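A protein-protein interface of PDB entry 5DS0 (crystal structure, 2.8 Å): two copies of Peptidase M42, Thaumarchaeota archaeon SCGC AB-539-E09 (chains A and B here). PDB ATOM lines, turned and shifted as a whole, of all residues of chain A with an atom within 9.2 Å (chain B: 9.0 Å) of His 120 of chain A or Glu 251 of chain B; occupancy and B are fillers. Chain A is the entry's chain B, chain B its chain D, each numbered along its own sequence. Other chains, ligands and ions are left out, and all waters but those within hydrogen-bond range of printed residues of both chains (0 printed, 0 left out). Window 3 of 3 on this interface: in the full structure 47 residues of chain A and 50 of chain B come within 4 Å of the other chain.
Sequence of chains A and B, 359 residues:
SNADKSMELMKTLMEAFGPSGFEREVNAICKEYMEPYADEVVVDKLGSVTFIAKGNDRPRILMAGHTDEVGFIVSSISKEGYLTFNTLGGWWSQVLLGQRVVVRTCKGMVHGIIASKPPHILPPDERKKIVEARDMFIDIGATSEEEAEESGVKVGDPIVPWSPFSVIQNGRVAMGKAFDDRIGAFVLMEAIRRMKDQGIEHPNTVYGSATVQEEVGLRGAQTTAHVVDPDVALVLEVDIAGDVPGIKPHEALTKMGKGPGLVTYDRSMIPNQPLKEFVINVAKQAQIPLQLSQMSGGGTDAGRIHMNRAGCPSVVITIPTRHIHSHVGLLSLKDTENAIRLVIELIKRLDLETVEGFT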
ATOM      1  N   SER A 116      23.529   2.612  17.834  1.00  0.00           N
ATOM      2  CA  SER A 116      22.486   1.869  18.528  1.00  0.00           C
ATOM      3  C   SER A 116      22.322   2.429  19.924  1.00  0.00           C
ATOM      4  O   SER A 116      23.023   3.363  20.311  1.00  0.00           O
ATOM      5  CB  SER A 116      22.849   0.392  18.617  1.00  0.00           C
ATOM      6  OG  SER A 116      23.906   0.191  19.535  1.00  0.00           O
ATOM      7  N   LYS A 117      21.390   1.860  20.675  1.00  0.00           N
ATOM      8  CA  LYS A 117      21.322   2.129  22.096  1.00  0.00           C
ATOM      9  C   LYS A 117      22.640   1.676  22.717  1.00  0.00           C
ATOM     10  O   LYS A 117      23.102   0.566  22.424  1.00  0.00           O
ATOM     11  CB  LYS A 117      20.160   1.387  22.747  1.00  0.00           C
ATOM     12  CG  LYS A 117      18.841   2.136  22.660  1.00  0.00           C
ATOM     13  CD  LYS A 117      17.712   1.328  23.284  1.00  0.00           C
ATOM     14  CE  LYS A 117      17.177   0.258  22.330  1.00  0.00           C
ATOM     15  NZ  LYS A 117      16.106  -0.554  22.970  1.00  0.00           N
ATOM     16  N   PRO A 118      23.250   2.532  23.568  1.00  0.00           N
ATOM     17  CA  PRO A 118      24.500   2.186  24.251  1.00  0.00           C
ATOM     18  C   PRO A 118      24.257   1.071  25.245  1.00  0.00           C
ATOM     19  O   PRO A 118      23.211   1.065  25.876  1.00  0.00           O
ATOM     20  CB  PRO A 118      24.891   3.469  24.994  1.00  0.00           C
ATOM     21  CG  PRO A 118      23.834   4.486  24.720  1.00  0.00           C
ATOM     22  CD  PRO A 118      22.688   3.815  24.035  1.00  0.00           C
ATOM     23  N   PRO A 119      25.214   0.142  25.396  1.00  0.00           N
ATOM     24  CA  PRO A 119      24.983  -1.063  26.226  1.00  0.00           C
ATOM     25  C   PRO A 119      24.752  -0.819  27.738  1.00  0.00           C
ATOM     26  O   PRO A 119      24.062  -1.612  28.375  1.00  0.00           O
ATOM     27  CB  PRO A 119      26.245  -1.915  25.992  1.00  0.00           C
ATOM     28  CG  PRO A 119      27.285  -0.950  25.540  1.00  0.00           C
ATOM     29  CD  PRO A 119      26.570   0.170  24.822  1.00  0.00           C
ATOM     30  N   HIS A 120      25.286   0.267  28.299  1.00  0.00           N
ATOM     31  CA  HIS A 120      25.107   0.549  29.734  1.00  0.00           C
ATOM     32  C   HIS A 120      23.654   0.954  30.128  1.00  0.00           C
ATOM     33  O   HIS A 120      23.333   0.949  31.312  1.00  0.00           O
ATOM     34  CB  HIS A 120      26.124   1.601  30.202  1.00  0.00           C
ATOM     35  CG  HIS A 120      25.702   3.010  29.917  1.00  0.00           C
ATOM     36  ND1 HIS A 120      25.170   3.835  30.885  1.00  0.00           N
ATOM     37  CD2 HIS A 120      25.707   3.731  28.770  1.00  0.00           C
ATOM     38  CE1 HIS A 120      24.875   5.007  30.350  1.00  0.00           C
ATOM     39  NE2 HIS A 120      25.191   4.969  29.068  1.00  0.00           N
ATOM     40  N   ILE A 121      22.808   1.315  29.149  1.00  0.00           N
ATOM     41  CA  ILE A 121      21.357   1.544  29.317  1.00  0.00           C
ATOM     42  C   ILE A 121      20.516   0.297  29.046  1.00  0.00           C
ATOM     43  O   ILE A 121      19.302   0.397  28.935  1.00  0.00           O
ATOM     44  CB  ILE A 121      20.876   2.671  28.271  1.00  0.00           C
ATOM     45  CG1 ILE A 121      19.750   3.572  28.803  1.00  0.00           C
ATOM     46  CG2 ILE A 121      20.397   2.121  26.897  1.00  0.00           C
ATOM     47  CD1 ILE A 121      19.534   4.874  28.023  1.00  0.00           C
ATOM     48  N   LEU A 122      21.149  -0.868  28.921  1.00  0.00           N
ATOM     49  CA  LEU A 122      20.440  -2.120  28.663  1.00  0.00           C
ATOM     50  C   LEU A 122      20.617  -3.044  29.856  1.00  0.00           C
ATOM     51  O   LEU A 122      21.548  -2.861  30.649  1.00  0.00           O
ATOM     52  CB  LEU A 122      20.992  -2.785  27.388  1.00  0.00           C
ATOM     53  CG  LEU A 122      20.733  -2.018  26.055  1.00  0.00           C
ATOM     54  CD1 LEU A 122      21.279  -2.502  24.706  1.00  0.00           C
ATOM     55  CD2 LEU A 122      19.260  -1.776  25.884  1.00  0.00           C
ATOM     56  N   PRO A 123      19.723  -4.039  29.997  1.00  0.00           N
ATOM     57  CA  PRO A 123      19.907  -5.035  31.060  1.00  0.00           C
ATOM     58  C   PRO A 123      21.202  -5.840  30.849  1.00  0.00           C
ATOM     59  O   PRO A 123      21.623  -6.003  29.706  1.00  0.00           O
ATOM     60  CB  PRO A 123      18.661  -5.936  30.935  1.00  0.00           C
ATOM     61  CG  PRO A 123      17.683  -5.172  30.100  1.00  0.00           C
ATOM     62  CD  PRO A 123      18.491  -4.271  29.218  1.00  0.00           C
ATOM     63  N   PRO A 124      21.831  -6.336  31.937  1.00  0.00           N
ATOM     64  CA  PRO A 124      23.101  -7.068  31.789  1.00  0.00           C
ATOM     65  C   PRO A 124      23.090  -8.241  30.792  1.00  0.00           C
ATOM     66  O   PRO A 124      24.085  -8.454  30.097  1.00  0.00           O
ATOM     67  CB  PRO A 124      23.412  -7.559  33.220  1.00  0.00           C
ATOM     68  CG  PRO A 124      22.209  -7.250  34.052  1.00  0.00           C
ATOM     69  CD  PRO A 124      21.458  -6.156  33.353  1.00  0.00           C
ATOM     70  N   GLU A 126      21.315  -8.481  28.049  1.00  0.00           N
ATOM     71  CA  GLU A 126      21.121  -7.976  26.679  1.00  0.00           C
ATOM     72  C   GLU A 126      22.374  -7.316  26.073  1.00  0.00           C
ATOM     73  O   GLU A 126      22.417  -7.058  24.874  1.00  0.00           O
ATOM     74  CB  GLU A 126      19.951  -6.983  26.641  1.00  0.00           C
ATOM     75  CG  GLU A 126      18.649  -7.508  27.254  1.00  0.00           C
ATOM     76  CD  GLU A 126      17.820  -8.366  26.310  1.00  0.00           C
ATOM     77  OE1 GLU A 126      16.591  -8.457  26.530  1.00  0.00           O
ATOM     78  OE2 GLU A 126      18.370  -8.947  25.352  1.00  0.00           O
ATOM     79  N   ARG A 127      23.391  -7.060  26.893  1.00  0.00           N
ATOM     80  CA  ARG A 127      24.653  -6.465  26.422  1.00  0.00           C
ATOM     81  C   ARG A 127      25.520  -7.458  25.641  1.00  0.00           C
ATOM     82  O   ARG A 127      26.223  -7.074  24.710  1.00  0.00           O
ATOM     83  CB  ARG A 127      25.466  -5.918  27.604  1.00  0.00           C
ATOM     84  CG  ARG A 127      24.757  -4.837  28.403  1.00  0.00           C
ATOM     85  CD  ARG A 127      25.703  -4.068  29.315  1.00  0.00           C
ATOM     86  NE  ARG A 127      24.894  -3.213  30.181  1.00  0.00           N
ATOM     87  CZ  ARG A 127      24.633  -3.468  31.465  1.00  0.00           C
ATOM     88  NH1 ARG A 127      23.848  -2.658  32.172  1.00  0.00           N
ATOM     89  NH2 ARG A 127      25.171  -4.526  32.066  1.00  0.00           N
ATOM     90  N   TRP B  92      33.695  -1.233  23.548  1.00  0.00           N
ATOM     91  CA  TRP B  92      32.646  -2.203  23.241  1.00  0.00           C
ATOM     92  C   TRP B  92      33.039  -2.960  21.967  1.00  0.00           C
ATOM     93  O   TRP B  92      33.320  -2.342  20.940  1.00  0.00           O
ATOM     94  CB  TRP B  92      31.332  -1.482  23.035  1.00  0.00           C
ATOM     95  CG  TRP B  92      30.152  -2.361  22.908  1.00  0.00           C
ATOM     96  CD1 TRP B  92      30.032  -3.642  23.347  1.00  0.00           C
ATOM     97  CD2 TRP B  92      28.888  -2.011  22.349  1.00  0.00           C
ATOM     98  NE1 TRP B  92      28.778  -4.127  23.071  1.00  0.00           N
ATOM     99  CE2 TRP B  92      28.055  -3.136  22.460  1.00  0.00           C
ATOM    100  CE3 TRP B  92      28.384  -0.861  21.739  1.00  0.00           C
ATOM    101  CZ2 TRP B  92      26.744  -3.141  21.993  1.00  0.00           C
ATOM    102  CZ3 TRP B  92      27.088  -0.867  21.276  1.00  0.00           C
ATOM    103  CH2 TRP B  92      26.281  -1.994  21.407  1.00  0.00           C
ATOM    104  N   ASP B 239      30.151  13.581  28.927  1.00  0.00           N
ATOM    105  CA  ASP B 239      29.032  12.852  29.482  1.00  0.00           C
ATOM    106  C   ASP B 239      28.450  12.025  28.350  1.00  0.00           C
ATOM    107  O   ASP B 239      28.431  12.475  27.201  1.00  0.00           O
ATOM    108  CB  ASP B 239      27.973  13.834  29.993  1.00  0.00           C
ATOM    109  CG  ASP B 239      27.409  13.455  31.370  1.00  0.00           C
ATOM    110  OD1 ASP B 239      27.165  12.251  31.621  1.00  0.00           O
ATOM    111  OD2 ASP B 239      27.174  14.397  32.173  1.00  0.00           O
ATOM    112  N   ILE B 240      27.997  10.815  28.655  1.00  0.00           N
ATOM    113  CA  ILE B 240      27.328  10.012  27.659  1.00  0.00           C
ATOM    114  C   ILE B 240      25.983  10.672  27.410  1.00  0.00           C
ATOM    115  O   ILE B 240      25.205  10.844  28.340  1.00  0.00           O
ATOM    116  CB  ILE B 240      27.115   8.559  28.114  1.00  0.00           C
ATOM    117  CG1 ILE B 240      28.457   7.824  28.313  1.00  0.00           C
ATOM    118  CG2 ILE B 240      26.272   7.817  27.085  1.00  0.00           C
ATOM    119  CD1 ILE B 240      28.848   7.600  29.765  1.00  0.00           C
ATOM    120  N   ALA B 241      25.728  11.069  26.168  1.00  0.00           N
ATOM    121  CA  ALA B 241      24.523  11.798  25.851  1.00  0.00           C
ATOM    122  C   ALA B 241      23.437  10.841  25.432  1.00  0.00           C
ATOM    123  O   ALA B 241      23.602  10.096  24.452  1.00  0.00           O
ATOM    124  CB  ALA B 241      24.787  12.797  24.752  1.00  0.00           C
ATOM    125  N   GLY B 242      22.326  10.874  26.172  1.00  0.00           N
ATOM    126  CA  GLY B 242      21.163  10.029  25.903  1.00  0.00           C
ATOM    127  C   GLY B 242      20.155  10.678  24.962  1.00  0.00           C
ATOM    128  O   GLY B 242      19.037  11.002  25.361  1.00  0.00           O
ATOM    129  N   VAL B 244      19.518   9.127  22.040  1.00  0.00           N
ATOM    130  CA  VAL B 244      19.254   7.975  21.207  1.00  0.00           C
ATOM    131  C   VAL B 244      17.889   7.347  21.586  1.00  0.00           C
ATOM    132  O   VAL B 244      17.603   7.184  22.766  1.00  0.00           O
ATOM    133  CB  VAL B 244      20.419   6.946  21.439  1.00  0.00           C
ATOM    134  CG1 VAL B 244      20.249   5.816  20.479  1.00  0.00           C
ATOM    135  CG2 VAL B 244      21.870   7.504  21.316  1.00  0.00           C
ATOM    136  N   GLY B 246      14.596   5.393  22.747  1.00  0.00           N
ATOM    137  CA  GLY B 246      14.457   4.414  23.824  1.00  0.00           C
ATOM    138  C   GLY B 246      14.783   5.022  25.178  1.00  0.00           C
ATOM    139  O   GLY B 246      15.952   5.100  25.572  1.00  0.00           O
ATOM    140  N   LYS B 248      16.605   3.895  29.954  1.00  0.00           N
ATOM    141  CA  LYS B 248      15.722   4.933  29.447  1.00  0.00           C
ATOM    142  C   LYS B 248      16.397   6.333  29.700  1.00  0.00           C
ATOM    143  O   LYS B 248      17.620   6.424  29.951  1.00  0.00           O
ATOM    144  CB  LYS B 248      14.356   4.807  30.166  1.00  0.00           C
ATOM    145  N   PRO B 249      15.602   7.425  29.682  1.00  0.00           N
ATOM    146  CA  PRO B 249      16.026   8.811  29.974  1.00  0.00           C
ATOM    147  C   PRO B 249      16.848   8.851  31.271  1.00  0.00           C
ATOM    148  O   PRO B 249      17.903   9.471  31.314  1.00  0.00           O
ATOM    149  CB  PRO B 249      14.695   9.613  30.042  1.00  0.00           C
ATOM    150  CG  PRO B 249      13.620   8.574  30.167  1.00  0.00           C
ATOM    151  CD  PRO B 249      14.144   7.297  29.608  1.00  0.00           C
ATOM    152  N   HIS B 250      16.420   8.104  32.284  1.00  0.00           N
ATOM    153  CA  HIS B 250      17.032   8.213  33.610  1.00  0.00           C
ATOM    154  C   HIS B 250      18.482   7.724  33.700  1.00  0.00           C
ATOM    155  O   HIS B 250      19.221   8.164  34.578  1.00  0.00           O
ATOM    156  CB  HIS B 250      16.191   7.491  34.663  1.00  0.00           C
ATOM    157  CG  HIS B 250      16.311   6.006  34.581  1.00  0.00           C
ATOM    158  ND1 HIS B 250      15.603   5.238  33.684  1.00  0.00           N
ATOM    159  CD2 HIS B 250      17.128   5.158  35.247  1.00  0.00           C
ATOM    160  CE1 HIS B 250      15.953   3.973  33.825  1.00  0.00           C
ATOM    161  NE2 HIS B 250      16.875   3.897  34.767  1.00  0.00           N
ATOM    162  N   GLU B 251      18.871   6.803  32.823  1.00  0.00           N
ATOM    163  CA  GLU B 251      20.244   6.265  32.814  1.00  0.00           C
ATOM    164  C   GLU B 251      21.251   7.228  32.144  1.00  0.00           C
ATOM    165  O   GLU B 251      22.444   7.170  32.426  1.00  0.00           O
ATOM    166  CB  GLU B 251      20.285   4.924  32.076  1.00  0.00           C
ATOM    167  CG  GLU B 251      19.289   3.836  32.527  1.00  0.00           C
ATOM    168  CD  GLU B 251      19.784   2.973  33.682  1.00  0.00           C
ATOM    169  OE1 GLU B 251      18.986   2.600  34.588  1.00  0.00           O
ATOM    170  OE2 GLU B 251      20.976   2.642  33.654  1.00  0.00           O
ATOM    171  N   ALA B 252      20.764   8.082  31.234  1.00  0.00           N
ATOM    172  CA  ALA B 252      21.575   9.112  30.565  1.00  0.00           C
ATOM    173  C   ALA B 252      20.762  10.398  30.465  1.00  0.00           C
ATOM    174  O   ALA B 252      20.056  10.645  29.494  1.00  0.00           O
ATOM    175  CB  ALA B 252      22.011   8.650  29.186  1.00  0.00           C
ATOM    176  N   LEU B 253      20.874  11.212  31.498  1.00  0.00           N
ATOM    177  CA  LEU B 253      20.085  12.422  31.605  1.00  0.00           C
ATOM    178  C   LEU B 253      20.433  13.502  30.568  1.00  0.00           C
ATOM    179  O   LEU B 253      19.555  14.280  30.207  1.00  0.00           O
ATOM    180  CB  LEU B 253      20.222  13.015  33.017  1.00  0.00           C
ATOM    181  CG  LEU B 253      19.498  12.235  34.119  1.00  0.00           C
ATOM    182  CD1 LEU B 253      20.156  12.471  35.472  1.00  0.00           C
ATOM    183  CD2 LEU B 253      18.006  12.550  34.149  1.00  0.00           C
ATOM    184  N   THR B 254      21.691  13.578  30.123  1.00  0.00           N
ATOM    185  CA  THR B 254      22.142  14.740  29.349  1.00  0.00           C
ATOM    186  C   THR B 254      21.796  14.639  27.879  1.00  0.00           C
ATOM    187  O   THR B 254      21.740  13.553  27.315  1.00  0.00           O
ATOM    188  CB  THR B 254      23.653  14.992  29.477  1.00  0.00           C
ATOM    189  OG1 THR B 254      24.366  13.817  29.119  1.00  0.00           O
ATOM    190  CG2 THR B 254      24.001  15.364  30.891  1.00  0.00           C
ATOM    191  N   TYR B 265      26.643  12.479  40.963  1.00  0.00           N
ATOM    192  CA  TYR B 265      27.111  11.218  41.523  1.00  0.00           C
ATOM    193  C   TYR B 265      27.767  10.374  40.437  1.00  0.00           C
ATOM    194  O   TYR B 265      27.257  10.298  39.330  1.00  0.00           O
ATOM    195  CB  TYR B 265      25.964  10.401  42.153  1.00  0.00           C
ATOM    196  CG  TYR B 265      26.385   8.974  42.448  1.00  0.00           C
ATOM    197  CD1 TYR B 265      27.243   8.700  43.498  1.00  0.00           C
ATOM    198  CD2 TYR B 265      25.982   7.915  41.634  1.00  0.00           C
ATOM    199  CE1 TYR B 265      27.660   7.406  43.762  1.00  0.00           C
ATOM    200  CE2 TYR B 265      26.399   6.614  41.887  1.00  0.00           C
ATOM    201  CZ  TYR B 265      27.237   6.371  42.956  1.00  0.00           C
ATOM    202  OH  TYR B 265      27.654   5.104  43.249  1.00  0.00           O
ATOM    203  N   SER B 293      23.445  15.692  36.001  1.00  0.00           N
ATOM    204  CA  SER B 293      23.800  14.398  35.435  1.00  0.00           C
ATOM    205  C   SER B 293      24.246  13.406  36.509  1.00  0.00           C
ATOM    206  O   SER B 293      24.636  13.791  37.605  1.00  0.00           O
ATOM    207  CB  SER B 293      24.922  14.601  34.430  1.00  0.00           C
ATOM    208  OG  SER B 293      25.557  13.378  34.117  1.00  0.00           O
ATOM    209  N   GLN B 294      24.212  12.123  36.168  1.00  0.00           N
ATOM    210  CA  GLN B 294      24.657  11.077  37.072  1.00  0.00           C
ATOM    211  C   GLN B 294      25.220   9.927  36.262  1.00  0.00           C
ATOM    212  O   GLN B 294      24.560   9.453  35.384  1.00  0.00           O
ATOM    213  CB  GLN B 294      23.470  10.606  37.907  1.00  0.00           C
ATOM    214  CG  GLN B 294      23.799  10.424  39.378  1.00  0.00           C
ATOM    215  CD  GLN B 294      22.572  10.231  40.251  1.00  0.00           C
ATOM    216  OE1 GLN B 294      22.107   9.108  40.451  1.00  0.00           O
ATOM    217  NE2 GLN B 294      22.036  11.338  40.781  1.00  0.00           N
ATOM    218  N   MET B 295      26.441   9.490  36.551  1.00  0.00           N
ATOM    219  CA  MET B 295      27.065   8.373  35.818  1.00  0.00           C
ATOM    220  C   MET B 295      27.193   7.190  36.738  1.00  0.00           C
ATOM    221  O   MET B 295      28.234   6.947  37.343  1.00  0.00           O
ATOM    222  CB  MET B 295      28.427   8.761  35.224  1.00  0.00           C
ATOM    223  CG  MET B 295      28.430  10.165  34.596  1.00  0.00           C
ATOM    224  SD  MET B 295      30.239  10.791  34.085  1.00  0.00           S
ATOM    225  CE  MET B 295      31.445   9.751  35.258  1.00  0.00           C
ATOM    226  N   SER B 296      26.098   6.451  36.854  1.00  0.00           N
ATOM    227  CA  SER B 296      26.017   5.192  37.637  1.00  0.00           C
ATOM    228  C   SER B 296      27.218   4.215  37.522  1.00  0.00           C
ATOM    229  O   SER B 296      27.614   3.592  38.513  1.00  0.00           O
ATOM    230  CB  SER B 296      24.720   4.456  37.251  1.00  0.00           C
ATOM    231  OG  SER B 296      24.836   3.072  37.455  1.00  0.00           O
ATOM    232  N   GLY B 297      27.783   4.081  36.322  1.00  0.00           N
ATOM    233  CA  GLY B 297      28.842   3.105  36.088  1.00  0.00           C
ATOM    234  C   GLY B 297      30.042   3.622  35.313  1.00  0.00           C
ATOM    235  O   GLY B 297      30.462   3.017  34.318  1.00  0.00           O
ATOM    236  N   GLY B 298      30.610   4.726  35.774  1.00  0.00           N
ATOM    237  CA  GLY B 298      31.826   5.257  35.176  1.00  0.00           C
ATOM    238  C   GLY B 298      32.536   6.113  36.191  1.00  0.00           C
ATOM    239  O   GLY B 298      31.938   6.533  37.176  1.00  0.00           O
ATOM    240  N   THR B 321      28.373  14.289  24.911  1.00  0.00           N
ATOM    241  CA  THR B 321      29.009  13.789  23.711  1.00  0.00           C
ATOM    242  C   THR B 321      28.334  12.489  23.325  1.00  0.00           C
ATOM    243  O   THR B 321      28.065  11.658  24.175  1.00  0.00           O
ATOM    244  CB  THR B 321      30.493  13.508  23.980  1.00  0.00           C
ATOM    245  OG1 THR B 321      31.130  14.708  24.434  1.00  0.00           O
ATOM    246  CG2 THR B 321      31.199  13.011  22.728  1.00  0.00           C
ATOM    247  N   ILE B 324      30.978   8.128  22.592  1.00  0.00           N
ATOM    248  CA  ILE B 324      32.341   8.136  23.113  1.00  0.00           C
ATOM    249  C   ILE B 324      32.914   6.717  23.102  1.00  0.00           C
ATOM    250  O   ILE B 324      32.192   5.759  22.853  1.00  0.00           O
ATOM    251  CB  ILE B 324      32.425   8.717  24.519  1.00  0.00           C
ATOM    252  CG1 ILE B 324      31.600   7.883  25.494  1.00  0.00           C
ATOM    253  CG2 ILE B 324      31.958  10.159  24.512  1.00  0.00           C
ATOM    254  CD1 ILE B 324      31.934   8.152  26.946  1.00  0.00           C
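OE1 of Glu 251 of chain B is in hydrogen-bond range of NE2 of His 250 of chain B (2.5 Å). O of Ile 240 of chain B sits at hydrogen-bond distance from OG1 of Thr 254 of chain B, 3.2 Å away. O of Pro 119 of chain A lies within hydrogen-bond range of NE of Arg 127 of chain A.
Ser 116 of chain A touches Trp 92 of chain B (OG to CH2, 3.7 Å). Val 244 of chain B touches Ser 116 of chain A. Trp 92 of chain B touches Pro 119 of chain A. NE2 of His 120 of chain A touches CG2 of Ile 240 of chain B (3.6 Å). His 120 of chain A touches Glu 251 of chain B. Ile 121 of chain A touches Lys 248 of chain B. Glu 251 of chain B touches Ile 121 of chain A.
Of the printed residues of chain B, His 120 of chain A touches Ile 240 and Glu 251. Of chain A, only His 120 (3.7 Å) and Ile 121 (3.6 Å) come within 4 Å of Glu 251 of chain B. Of chain B, only Trp 92 comes within 4 Å of Pro 119 of chain A. Of chain B, only Lys 248 and Glu 251 come within 4 Å of Ile 121 of chain A. No residue of chain A comes within 4 Å of Ala 252 of chain B. Of the printed residues of chain A, Ile 240 of chain B touches His 120. Printed residues of chain A within 4 Å of Trp 92 of chain B: Ser 116 (3.7 Å) and Pro 119 (3.7 Å). Of the printed residues of chain B, Ser 116 of chain A touches Trp 92 and Val 244. Of the printed residues of chain A, Val 244 of chain B touches Ser 116. Tyr 265 of chain B touches none of the printed residues of chain A. The nearest printed residue of chain A that does not touch Val 244 of chain B is Lys 117 of chain A (4.1 Å).
Of the 23 printed residues of chain B, 5 touch a printed residue of chain A. Hydrophobic or aromatic side chains of chain B within 4 Å of the printed part of chain A: Trp 92, Ile 240 and Val 244. Along chain B the printed residues that touch a printed residue of chain A span positions 92 to 251.
No position is printed for both chains. Of the 7 pairs that touch across the chains among the printed residues, none has its exchanged pair printed and touching as well.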
